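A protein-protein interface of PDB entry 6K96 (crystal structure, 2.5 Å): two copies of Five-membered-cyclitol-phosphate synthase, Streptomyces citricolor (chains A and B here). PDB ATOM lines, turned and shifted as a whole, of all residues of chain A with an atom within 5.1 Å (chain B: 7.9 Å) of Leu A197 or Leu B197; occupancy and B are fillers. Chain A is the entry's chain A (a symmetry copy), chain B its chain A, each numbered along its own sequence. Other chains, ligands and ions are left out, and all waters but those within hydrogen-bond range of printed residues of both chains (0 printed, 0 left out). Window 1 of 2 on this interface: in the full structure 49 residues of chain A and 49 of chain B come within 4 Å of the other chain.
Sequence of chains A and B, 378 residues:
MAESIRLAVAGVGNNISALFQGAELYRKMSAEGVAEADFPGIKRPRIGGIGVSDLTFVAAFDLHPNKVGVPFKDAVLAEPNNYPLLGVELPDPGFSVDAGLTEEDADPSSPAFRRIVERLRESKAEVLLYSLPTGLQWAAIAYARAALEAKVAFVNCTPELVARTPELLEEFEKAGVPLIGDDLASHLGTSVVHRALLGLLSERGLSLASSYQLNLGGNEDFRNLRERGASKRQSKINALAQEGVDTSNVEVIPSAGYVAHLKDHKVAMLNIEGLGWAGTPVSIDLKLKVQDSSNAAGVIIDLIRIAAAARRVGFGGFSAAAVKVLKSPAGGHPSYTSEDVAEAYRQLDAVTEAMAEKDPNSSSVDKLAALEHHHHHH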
ATOM      1  N   VAL A 193       4.251 -25.590  16.696  1.00  0.00           N
ATOM      2  CA  VAL A 193       4.812 -24.856  17.856  1.00  0.00           C
ATOM      3  C   VAL A 193       3.781 -24.887  18.966  1.00  0.00           C
ATOM      4  O   VAL A 193       4.137 -25.233  20.070  1.00  0.00           O
ATOM      5  CB  VAL A 193       5.262 -23.428  17.533  1.00  0.00           C
ATOM      6  CG1 VAL A 193       5.604 -22.650  18.787  1.00  0.00           C
ATOM      7  CG2 VAL A 193       6.453 -23.409  16.594  1.00  0.00           C
ATOM      8  N   HIS A 194       2.521 -24.573  18.671  1.00  0.00           N
ATOM      9  CA  HIS A 194       1.459 -24.486  19.710  1.00  0.00           C
ATOM     10  C   HIS A 194       1.380 -25.838  20.410  1.00  0.00           C
ATOM     11  O   HIS A 194       1.379 -25.845  21.664  1.00  0.00           O
ATOM     12  CB  HIS A 194       0.129 -24.045  19.127  1.00  0.00           C
ATOM     13  CG  HIS A 194      -0.895 -23.686  20.139  1.00  0.00           C
ATOM     14  ND1 HIS A 194      -2.119 -23.142  19.784  1.00  0.00           N
ATOM     15  CD2 HIS A 194      -0.883 -23.727  21.486  1.00  0.00           C
ATOM     16  CE1 HIS A 194      -2.835 -22.913  20.870  1.00  0.00           C
ATOM     17  NE2 HIS A 194      -2.073 -23.221  21.935  1.00  0.00           N
ATOM     18  N   ARG A 195       1.380 -26.923  19.639  1.00  0.00           N
ATOM     19  CA  ARG A 195       1.072 -28.286  20.159  1.00  0.00           C
ATOM     20  C   ARG A 195       2.237 -28.798  21.005  1.00  0.00           C
ATOM     21  O   ARG A 195       1.978 -29.530  21.959  1.00  0.00           O
ATOM     22  CB  ARG A 195       0.744 -29.298  19.047  1.00  0.00           C
ATOM     23  CG  ARG A 195       1.443 -30.662  19.161  1.00  0.00           C
ATOM     24  CD  ARG A 195       0.674 -31.796  18.435  1.00  0.00           C
ATOM     25  NE  ARG A 195      -0.455 -31.234  17.652  1.00  0.00           N
ATOM     26  CZ  ARG A 195      -0.409 -30.839  16.387  1.00  0.00           C
ATOM     27  NH1 ARG A 195       0.725 -30.947  15.706  1.00  0.00           N
ATOM     28  NH2 ARG A 195      -1.502 -30.351  15.809  1.00  0.00           N
ATOM     29  N   ALA A 196       3.471 -28.464  20.619  1.00  0.00           N
ATOM     30  CA  ALA A 196       4.703 -28.862  21.324  1.00  0.00           C
ATOM     31  C   ALA A 196       4.643 -28.246  22.728  1.00  0.00           C
ATOM     32  O   ALA A 196       4.972 -28.960  23.703  1.00  0.00           O
ATOM     33  CB  ALA A 196       5.910 -28.422  20.533  1.00  0.00           C
ATOM     34  N   LEU A 197       4.216 -26.981  22.820  1.00  0.00           N
ATOM     35  CA  LEU A 197       4.175 -26.242  24.106  1.00  0.00           C
ATOM     36  C   LEU A 197       3.066 -26.831  24.978  1.00  0.00           C
ATOM     37  O   LEU A 197       3.287 -26.962  26.198  1.00  0.00           O
ATOM     38  CB  LEU A 197       3.932 -24.753  23.860  1.00  0.00           C
ATOM     39  CG  LEU A 197       5.037 -24.001  23.118  1.00  0.00           C
ATOM     40  CD1 LEU A 197       4.675 -22.513  23.005  1.00  0.00           C
ATOM     41  CD2 LEU A 197       6.379 -24.177  23.768  1.00  0.00           C
ATOM     42  N   LEU A 198       1.918 -27.185  24.399  1.00  0.00           N
ATOM     43  CA  LEU A 198       0.800 -27.753  25.207  1.00  0.00           C
ATOM     44  C   LEU A 198       1.208 -29.144  25.670  1.00  0.00           C
ATOM     45  O   LEU A 198       0.865 -29.487  26.821  1.00  0.00           O
ATOM     46  CB  LEU A 198      -0.492 -27.791  24.398  1.00  0.00           C
ATOM     47  CG  LEU A 198      -1.220 -26.468  24.263  1.00  0.00           C
ATOM     48  CD1 LEU A 198      -2.252 -26.558  23.149  1.00  0.00           C
ATOM     49  CD2 LEU A 198      -1.881 -26.137  25.553  1.00  0.00           C
ATOM     50  N   GLY A 199       1.987 -29.850  24.836  1.00  0.00           N
ATOM     51  CA  GLY A 199       2.560 -31.185  25.108  1.00  0.00           C
ATOM     52  C   GLY A 199       3.426 -31.131  26.358  1.00  0.00           C
ATOM     53  O   GLY A 199       3.293 -32.000  27.227  1.00  0.00           O
ATOM     54  N   LEU A 200       4.285 -30.106  26.428  1.00  0.00           N
ATOM     55  CA  LEU A 200       5.185 -29.800  27.551  1.00  0.00           C
ATOM     56  C   LEU A 200       4.366 -29.634  28.822  1.00  0.00           C
ATOM     57  O   LEU A 200       4.753 -30.287  29.815  1.00  0.00           O
ATOM     58  CB  LEU A 200       5.996 -28.548  27.242  1.00  0.00           C
ATOM     59  CG  LEU A 200       7.483 -28.731  27.526  1.00  0.00           C
ATOM     60  CD1 LEU A 200       8.101 -29.673  26.484  1.00  0.00           C
ATOM     61  CD2 LEU A 200       8.201 -27.393  27.563  1.00  0.00           C
ATOM     62  N   LEU A 201       3.291 -28.848  28.787  1.00  0.00           N
ATOM     63  CA  LEU A 201       2.509 -28.563  30.007  1.00  0.00           C
ATOM     64  C   LEU A 201       1.920 -29.836  30.613  1.00  0.00           C
ATOM     65  O   LEU A 201       1.961 -29.962  31.885  1.00  0.00           O
ATOM     66  CB  LEU A 201       1.464 -27.480  29.758  1.00  0.00           C
ATOM     67  CG  LEU A 201       1.968 -26.103  30.206  1.00  0.00           C
ATOM     68  CD1 LEU A 201       3.111 -25.630  29.321  1.00  0.00           C
ATOM     69  CD2 LEU A 201       0.862 -25.078  30.227  1.00  0.00           C
ATOM     70  N   LEU A 270       0.526 -16.558  20.150  1.00  0.00           N
ATOM     71  CA  LEU A 270      -0.232 -17.487  21.004  1.00  0.00           C
ATOM     72  C   LEU A 270       0.015 -17.183  22.479  1.00  0.00           C
ATOM     73  O   LEU A 270       0.945 -16.403  22.839  1.00  0.00           O
ATOM     74  CB  LEU A 270      -0.009 -18.929  20.549  1.00  0.00           C
ATOM     75  CG  LEU A 270       1.368 -19.548  20.757  1.00  0.00           C
ATOM     76  CD1 LEU A 270       1.449 -20.245  22.122  1.00  0.00           C
ATOM     77  CD2 LEU A 270       1.724 -20.552  19.652  1.00  0.00           C
ATOM     78  N   ILE A 272      -0.663 -19.203  26.343  1.00  0.00           N
ATOM     79  CA  ILE A 272      -1.005 -20.396  27.157  1.00  0.00           C
ATOM     80  C   ILE A 272      -1.046 -19.924  28.586  1.00  0.00           C
ATOM     81  O   ILE A 272      -0.084 -19.344  29.006  1.00  0.00           O
ATOM     82  CB  ILE A 272       0.002 -21.539  26.954  1.00  0.00           C
ATOM     83  CG1 ILE A 272      -0.023 -22.045  25.506  1.00  0.00           C
ATOM     84  CG2 ILE A 272      -0.278 -22.665  27.935  1.00  0.00           C
ATOM     85  CD1 ILE A 272       1.185 -22.756  25.033  1.00  0.00           C
ATOM     86  N   ILE A 284       2.524 -18.155  29.192  1.00  0.00           N
ATOM     87  CA  ILE A 284       3.420 -18.167  27.992  1.00  0.00           C
ATOM     88  C   ILE A 284       2.804 -17.254  26.924  1.00  0.00           C
ATOM     89  O   ILE A 284       1.611 -17.359  26.661  1.00  0.00           O
ATOM     90  CB  ILE A 284       3.629 -19.588  27.418  1.00  0.00           C
ATOM     91  CG1 ILE A 284       4.458 -20.491  28.327  1.00  0.00           C
ATOM     92  CG2 ILE A 284       4.193 -19.542  25.996  1.00  0.00           C
ATOM     93  CD1 ILE A 284       4.868 -21.782  27.677  1.00  0.00           C
ATOM     94  N   LEU A 286       3.793 -15.897  22.978  1.00  0.00           N
ATOM     95  CA  LEU A 286       4.704 -16.305  21.900  1.00  0.00           C
ATOM     96  C   LEU A 286       4.325 -15.565  20.605  1.00  0.00           C
ATOM     97  O   LEU A 286       3.175 -15.269  20.438  1.00  0.00           O
ATOM     98  CB  LEU A 286       4.696 -17.840  21.798  1.00  0.00           C
ATOM     99  CG  LEU A 286       5.539 -18.361  20.639  1.00  0.00           C
ATOM    100  CD1 LEU A 286       6.238 -19.675  20.932  1.00  0.00           C
ATOM    101  CD2 LEU A 286       4.680 -18.469  19.398  1.00  0.00           C
ATOM    102  N   LEU B 188       8.198 -26.439  35.406  1.00  0.00           N
ATOM    103  CA  LEU B 188       8.209 -25.963  34.014  1.00  0.00           C
ATOM    104  C   LEU B 188       9.123 -24.762  33.934  1.00  0.00           C
ATOM    105  O   LEU B 188       8.624 -23.653  34.139  1.00  0.00           O
ATOM    106  CB  LEU B 188       6.823 -25.517  33.549  1.00  0.00           C
ATOM    107  CG  LEU B 188       6.865 -25.032  32.096  1.00  0.00           C
ATOM    108  CD1 LEU B 188       7.093 -26.239  31.206  1.00  0.00           C
ATOM    109  CD2 LEU B 188       5.630 -24.226  31.691  1.00  0.00           C
ATOM    110  N   THR B 190      12.417 -22.235  32.314  1.00  0.00           N
ATOM    111  CA  THR B 190      12.897 -21.535  31.129  1.00  0.00           C
ATOM    112  C   THR B 190      13.478 -22.536  30.147  1.00  0.00           C
ATOM    113  O   THR B 190      13.155 -22.478  28.911  1.00  0.00           O
ATOM    114  CB  THR B 190      13.936 -20.512  31.549  1.00  0.00           C
ATOM    115  OG1 THR B 190      13.367 -19.821  32.673  1.00  0.00           O
ATOM    116  CG2 THR B 190      14.290 -19.592  30.402  1.00  0.00           C
ATOM    117  N   SER B 191      14.325 -23.380  30.690  1.00  0.00           N
ATOM    118  CA  SER B 191      15.243 -24.295  29.975  1.00  0.00           C
ATOM    119  C   SER B 191      14.479 -25.373  29.193  1.00  0.00           C
ATOM    120  O   SER B 191      14.858 -25.756  28.097  1.00  0.00           O
ATOM    121  CB  SER B 191      16.136 -24.970  31.029  1.00  0.00           C
ATOM    122  OG  SER B 191      17.422 -24.446  30.925  1.00  0.00           O
ATOM    123  N   VAL B 192      13.503 -25.959  29.855  1.00  0.00           N
ATOM    124  CA  VAL B 192      12.757 -27.066  29.247  1.00  0.00           C
ATOM    125  C   VAL B 192      11.921 -26.472  28.094  1.00  0.00           C
ATOM    126  O   VAL B 192      11.860 -27.131  27.040  1.00  0.00           O
ATOM    127  CB  VAL B 192      11.929 -27.798  30.307  1.00  0.00           C
ATOM    128  CG1 VAL B 192      10.799 -26.925  30.847  1.00  0.00           C
ATOM    129  CG2 VAL B 192      11.372 -29.089  29.723  1.00  0.00           C
ATOM    130  N   VAL B 193      11.403 -25.232  28.228  1.00  0.00           N
ATOM    131  CA  VAL B 193      10.669 -24.555  27.132  1.00  0.00           C
ATOM    132  C   VAL B 193      11.665 -24.236  26.035  1.00  0.00           C
ATOM    133  O   VAL B 193      11.390 -24.558  24.901  1.00  0.00           O
ATOM    134  CB  VAL B 193       9.890 -23.314  27.576  1.00  0.00           C
ATOM    135  CG1 VAL B 193       9.356 -22.533  26.394  1.00  0.00           C
ATOM    136  CG2 VAL B 193       8.741 -23.667  28.500  1.00  0.00           C
ATOM    137  N   HIS B 194      12.814 -23.654  26.371  1.00  0.00           N
ATOM    138  CA  HIS B 194      13.812 -23.221  25.355  1.00  0.00           C
ATOM    139  C   HIS B 194      14.208 -24.445  24.538  1.00  0.00           C
ATOM    140  O   HIS B 194      14.197 -24.340  23.289  1.00  0.00           O
ATOM    141  CB  HIS B 194      15.002 -22.524  25.990  1.00  0.00           C
ATOM    142  CG  HIS B 194      15.897 -21.839  25.025  1.00  0.00           C
ATOM    143  ND1 HIS B 194      16.957 -21.049  25.441  1.00  0.00           N
ATOM    144  CD2 HIS B 194      15.880 -21.762  23.680  1.00  0.00           C
ATOM    145  CE1 HIS B 194      17.584 -20.557  24.388  1.00  0.00           C
ATOM    146  NE2 HIS B 194      16.908 -20.944  23.291  1.00  0.00           N
ATOM    147  N   ARG B 195      14.479 -25.562  25.210  1.00  0.00           N
ATOM    148  CA  ARG B 195      15.103 -26.757  24.574  1.00  0.00           C
ATOM    149  C   ARG B 195      14.087 -27.459  23.673  1.00  0.00           C
ATOM    150  O   ARG B 195      14.504 -28.018  22.661  1.00  0.00           O
ATOM    151  CB  ARG B 195      15.677 -27.755  25.595  1.00  0.00           C
ATOM    152  CG  ARG B 195      15.329 -29.233  25.351  1.00  0.00           C
ATOM    153  CD  ARG B 195      16.357 -30.206  25.982  1.00  0.00           C
ATOM    154  NE  ARG B 195      17.325 -29.460  26.824  1.00  0.00           N
ATOM    155  CZ  ARG B 195      17.199 -29.202  28.119  1.00  0.00           C
ATOM    156  NH1 ARG B 195      16.132 -29.641  28.775  1.00  0.00           N
ATOM    157  NH2 ARG B 195      18.148 -28.518  28.750  1.00  0.00           N
ATOM    158  N   ALA B 196      12.813 -27.470  24.073  1.00  0.00           N
ATOM    159  CA  ALA B 196      11.707 -28.090  23.322  1.00  0.00           C
ATOM    160  C   ALA B 196      11.600 -27.355  21.980  1.00  0.00           C
ATOM    161  O   ALA B 196      11.443 -28.037  20.941  1.00  0.00           O
ATOM    162  CB  ALA B 196      10.438 -28.028  24.136  1.00  0.00           C
ATOM    163  N   LEU B 197      11.707 -26.022  22.005  1.00  0.00           N
ATOM    164  CA  LEU B 197      11.553 -25.182  20.791  1.00  0.00           C
ATOM    165  C   LEU B 197      12.763 -25.406  19.882  1.00  0.00           C
ATOM    166  O   LEU B 197      12.567 -25.477  18.652  1.00  0.00           O
ATOM    167  CB  LEU B 197      11.431 -23.707  21.171  1.00  0.00           C
ATOM    168  CG  LEU B 197      10.186 -23.314  21.965  1.00  0.00           C
ATOM    169  CD1 LEU B 197      10.178 -21.800  22.215  1.00  0.00           C
ATOM    170  CD2 LEU B 197       8.919 -23.751  21.288  1.00  0.00           C
ATOM    171  N   LEU B 198      13.968 -25.522  20.440  1.00  0.00           N
ATOM    172  CA  LEU B 198      15.182 -25.727  19.597  1.00  0.00           C
ATOM    173  C   LEU B 198      15.118 -27.128  19.007  1.00  0.00           C
ATOM    174  O   LEU B 198      15.521 -27.274  17.834  1.00  0.00           O
ATOM    175  CB  LEU B 198      16.453 -25.523  20.413  1.00  0.00           C
ATOM    176  CG  LEU B 198      16.841 -24.080  20.674  1.00  0.00           C
ATOM    177  CD1 LEU B 198      17.876 -24.018  21.787  1.00  0.00           C
ATOM    178  CD2 LEU B 198      17.388 -23.486  19.425  1.00  0.00           C
ATOM    179  N   GLY B 199      14.542 -28.074  19.765  1.00  0.00           N
ATOM    180  CA  GLY B 199      14.307 -29.477  19.370  1.00  0.00           C
ATOM    181  C   GLY B 199      13.440 -29.523  18.120  1.00  0.00           C
ATOM    182  O   GLY B 199      13.770 -30.253  17.178  1.00  0.00           O
ATOM    183  N   LEU B 200      12.358 -28.736  18.132  1.00  0.00           N
ATOM    184  CA  LEU B 200      11.398 -28.557  17.031  1.00  0.00           C
ATOM    185  C   LEU B 200      12.138 -28.085  15.789  1.00  0.00           C
ATOM    186  O   LEU B 200      11.910 -28.722  14.738  1.00  0.00           O
ATOM    187  CB  LEU B 200      10.311 -27.571  17.442  1.00  0.00           C
ATOM    188  CG  LEU B 200       8.910 -28.083  17.126  1.00  0.00           C
ATOM    189  CD1 LEU B 200       8.550 -29.236  18.073  1.00  0.00           C
ATOM    190  CD2 LEU B 200       7.889 -26.962  17.201  1.00  0.00           C
ATOM    191  N   LEU B 201      12.991 -27.068  15.906  1.00  0.00           N
ATOM    192  CA  LEU B 201      13.667 -26.495  14.725  1.00  0.00           C
ATOM    193  C   LEU B 201      14.540 -27.529  14.014  1.00  0.00           C
ATOM    194  O   LEU B 201      14.517 -27.547  12.736  1.00  0.00           O
ATOM    195  CB  LEU B 201      14.422 -25.218  15.081  1.00  0.00           C
ATOM    196  CG  LEU B 201      13.594 -23.969  14.752  1.00  0.00           C
ATOM    197  CD1 LEU B 201      12.381 -23.869  15.664  1.00  0.00           C
ATOM    198  CD2 LEU B 201      14.418 -22.710  14.836  1.00  0.00           C
ATOM    199  N   SER B 202      15.251 -28.378  14.753  1.00  0.00           N
ATOM    200  CA  SER B 202      16.238 -29.292  14.129  1.00  0.00           C
ATOM    201  C   SER B 202      15.576 -30.628  13.750  1.00  0.00           C
ATOM    202  O   SER B 202      15.987 -31.192  12.720  1.00  0.00           O
ATOM    203  CB  SER B 202      17.384 -29.477  15.042  1.00  0.00           C
ATOM    204  OG  SER B 202      16.825 -29.859  16.268  1.00  0.00           O
ATOM    205  N   GLU B 203      14.594 -31.113  14.523  1.00  0.00           N
ATOM    206  CA  GLU B 203      13.677 -32.231  14.170  1.00  0.00           C
ATOM    207  C   GLU B 203      13.134 -31.965  12.750  1.00  0.00           C
ATOM    208  O   GLU B 203      13.230 -32.868  11.937  1.00  0.00           O
ATOM    209  CB  GLU B 203      12.563 -32.394  15.226  1.00  0.00           C
ATOM    210  CG  GLU B 203      11.913 -33.786  15.334  1.00  0.00           C
ATOM    211  CD  GLU B 203      10.824 -34.269  14.322  1.00  0.00           C
ATOM    212  OE1 GLU B 203      10.937 -35.451  13.800  1.00  0.00           O
ATOM    213  OE2 GLU B 203       9.800 -33.526  14.064  1.00  0.00           O
ATOM    214  N   ARG B 204      12.666 -30.753  12.417  1.00  0.00           N
ATOM    215  CA  ARG B 204      11.999 -30.460  11.109  1.00  0.00           C
ATOM    216  C   ARG B 204      13.045 -29.982  10.105  1.00  0.00           C
ATOM    217  O   ARG B 204      12.691 -29.839   8.916  1.00  0.00           O
ATOM    218  CB  ARG B 204      10.842 -29.443  11.202  1.00  0.00           C
ATOM    219  CG  ARG B 204      10.015 -29.475  12.486  1.00  0.00           C
ATOM    220  CD  ARG B 204       8.629 -30.055  12.585  1.00  0.00           C
ATOM    221  NE  ARG B 204       7.879 -29.793  11.366  1.00  0.00           N
ATOM    222  CZ  ARG B 204       6.780 -30.473  10.977  1.00  0.00           C
ATOM    223  NH1 ARG B 204       6.234 -31.393  11.771  1.00  0.00           N
ATOM    224  NH2 ARG B 204       6.210 -30.211   9.799  1.00  0.00           N
ATOM    225  N   LEU B 208      19.457 -23.237  12.861  1.00  0.00           N
ATOM    226  CA  LEU B 208      19.517 -22.177  13.921  1.00  0.00           C
ATOM    227  C   LEU B 208      20.557 -21.111  13.534  1.00  0.00           C
ATOM    228  O   LEU B 208      21.615 -21.474  13.134  1.00  0.00           O
ATOM    229  CB  LEU B 208      19.886 -22.851  15.229  1.00  0.00           C
ATOM    230  CG  LEU B 208      19.799 -21.968  16.454  1.00  0.00           C
ATOM    231  CD1 LEU B 208      18.355 -21.632  16.772  1.00  0.00           C
ATOM    232  CD2 LEU B 208      20.420 -22.688  17.611  1.00  0.00           C
ATOM    233  N   SER B 211      20.033 -17.791  19.110  1.00  0.00           N
ATOM    234  CA  SER B 211      19.017 -17.876  20.186  1.00  0.00           C
ATOM    235  C   SER B 211      19.622 -17.168  21.419  1.00  0.00           C
ATOM    236  O   SER B 211      20.845 -17.067  21.512  1.00  0.00           O
ATOM    237  CB  SER B 211      18.652 -19.359  20.420  1.00  0.00           C
ATOM    238  OG  SER B 211      17.573 -19.616  21.335  1.00  0.00           O
ATOM    239  N   LEU B 270      12.792 -15.296  25.635  1.00  0.00           N
ATOM    240  CA  LEU B 270      13.743 -15.934  24.710  1.00  0.00           C
ATOM    241  C   LEU B 270      13.413 -15.568  23.265  1.00  0.00           C
ATOM    242  O   LEU B 270      12.319 -15.007  22.966  1.00  0.00           O
ATOM    243  CB  LEU B 270      13.881 -17.422  25.031  1.00  0.00           C
ATOM    244  CG  LEU B 270      12.692 -18.334  24.754  1.00  0.00           C
ATOM    245  CD1 LEU B 270      12.768 -18.905  23.332  1.00  0.00           C
ATOM    246  CD2 LEU B 270      12.602 -19.489  25.761  1.00  0.00           C
ATOM    247  N   ASN B 271      14.478 -15.609  22.473  1.00  0.00           N
ATOM    248  CA  ASN B 271      14.503 -15.337  21.029  1.00  0.00           C
ATOM    249  C   ASN B 271      15.134 -16.549  20.344  1.00  0.00           C
ATOM    250  O   ASN B 271      16.129 -17.075  20.885  1.00  0.00           O
ATOM    251  CB  ASN B 271      15.276 -14.072  20.735  1.00  0.00           C
ATOM    252  CG  ASN B 271      15.266 -13.778  19.259  1.00  0.00           C
ATOM    253  OD1 ASN B 271      16.332 -13.835  18.661  1.00  0.00           O
ATOM    254  ND2 ASN B 271      14.100 -13.457  18.685  1.00  0.00           N
ATOM    255  N   ILE B 272      14.518 -17.011  19.244  1.00  0.00           N
ATOM    256  CA  ILE B 272      15.130 -18.008  18.330  1.00  0.00           C
ATOM    257  C   ILE B 272      15.040 -17.415  16.950  1.00  0.00           C
ATOM    258  O   ILE B 272      13.961 -17.050  16.573  1.00  0.00           O
ATOM    259  CB  ILE B 272      14.432 -19.374  18.420  1.00  0.00           C
ATOM    260  CG1 ILE B 272      14.594 -19.986  19.817  1.00  0.00           C
ATOM    261  CG2 ILE B 272      14.966 -20.307  17.345  1.00  0.00           C
ATOM    262  CD1 ILE B 272      13.600 -21.008  20.212  1.00  0.00           C
ATOM    263  N   ILE B 284      11.141 -16.517  16.465  1.00  0.00           N
ATOM    264  CA  ILE B 284      10.287 -16.852  17.649  1.00  0.00           C
ATOM    265  C   ILE B 284      10.677 -15.916  18.801  1.00  0.00           C
ATOM    266  O   ILE B 284      11.862 -15.752  19.067  1.00  0.00           O
ATOM    267  CB  ILE B 284      10.435 -18.326  18.092  1.00  0.00           C
ATOM    268  CG1 ILE B 284       9.840 -19.319  17.097  1.00  0.00           C
ATOM    269  CG2 ILE B 284       9.893 -18.545  19.506  1.00  0.00           C
ATOM    270  CD1 ILE B 284       9.762 -20.723  17.624  1.00  0.00           C
ATOM    271  N   ASP B 285       9.687 -15.319  19.442  1.00  0.00           N
ATOM    272  CA  ASP B 285       9.839 -14.387  20.564  1.00  0.00           C
ATOM    273  C   ASP B 285       8.917 -14.981  21.610  1.00  0.00           C
ATOM    274  O   ASP B 285       7.767 -15.299  21.241  1.00  0.00           O
ATOM    275  CB  ASP B 285       9.565 -12.943  20.145  1.00  0.00           C
ATOM    276  CG  ASP B 285      10.698 -12.326  19.333  1.00  0.00           C
ATOM    277  OD1 ASP B 285      11.872 -12.494  19.699  1.00  0.00           O
ATOM    278  OD2 ASP B 285      10.428 -11.697  18.315  1.00  0.00           O
ATOM    279  N   LEU B 286       9.432 -15.196  22.842  1.00  0.00           N
ATOM    280  CA  LEU B 286       8.658 -15.906  23.868  1.00  0.00           C
ATOM    281  C   LEU B 286       8.861 -15.216  25.229  1.00  0.00           C
ATOM    282  O   LEU B 286       9.907 -14.667  25.434  1.00  0.00           O
ATOM    283  CB  LEU B 286       9.038 -17.397  23.834  1.00  0.00           C
ATOM    284  CG  LEU B 286       8.360 -18.208  24.932  1.00  0.00           C
ATOM    285  CD1 LEU B 286       7.996 -19.621  24.514  1.00  0.00           C
ATOM    286  CD2 LEU B 286       9.233 -18.216  26.167  1.00  0.00           C
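The backbone NH (N) of Leu B286 sits at hydrogen-bond distance from the backbone carbonyl oxygen (O) of Leu B270 (2.9 Å). The side-chain amide nitrogen of Asn B271 sits at hydrogen-bond distance from the side-chain carboxylate of Asp B285 (2.6 Å). O of Leu A270 lies within hydrogen-bond range of N of Leu A286.
Among the printed residues, pairs that only touch across the chains: Val A193 with Leu B200 (3.8 Å), Ala A196 with Leu B200 (3.7 Å), Leu A197 with Leu B197 (3.6 Å), Leu A200 with Leu B188 (3.98 Å), Leu A200 with Val B192 (3.7 Å), Leu A200 with Val B193 (3.8 Å), Leu A200 with Ala B196 (3.7 Å), Leu A201 with Leu B188 (3.7 Å), Leu A286 with Asp B285 (3.3 Å) and Leu A286 with Leu B286 (3.99 Å).
Printed residues of chain B within 4 Å of Val A193: Leu B200. Ala A196 touches just one residue of chain B: Leu B200 (3.7 Å). Of chain B, only Leu B197 comes within 4 Å of Leu A197. Of the printed residues of chain A, Leu B188 touches Leu A200 (3.98 Å) and Leu A201 (3.7 Å). Of the printed residues of chain A, Ala B196 touches Leu A200. Printed residues of chain A within 4 Å of Leu B197: Leu A197 (3.6 Å). Arg B204 touches none of the printed residues of chain A. Of the printed residues of chain A, Asp B285 touches Leu A286. The nearest residue of chain A that does not touch Leu B197 is Val A193 (4.3 Å). The nearest printed residue of chain A that does not touch Leu B200 is His A194 (6.1 Å).
Of the 24 printed residues of chain B, 8 touch a printed residue of chain A. Along chain B the printed residues that touch a printed residue of chain A span positions 188 to 286. Hydrophobic or aromatic side chains of chain A that line the printed part of chain B: Val A193, Ala A196, Leu A197, Leu A200, Leu A201 and Leu A286. Among the printed residues, 10 pairs touch across the chains. Among the printed residues, no Asp or Glu carboxylate lies within 4 Å of a Lys or Arg side-chain nitrogen of the other chain.
Val A193 touches Leu B200, and with the chains exchanged Leu A200 touches Val B193. Ala A196 touches Leu B200, and with the chains exchanged Leu A200 touches Ala B196. Leu B197 touches its own counterpart, Leu A197. Leu B286 touches its own counterpart, Leu A286. Of the 10 pairs that touch across the chains among the printed residues, 6 have their exchanged pair printed and touching as well.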
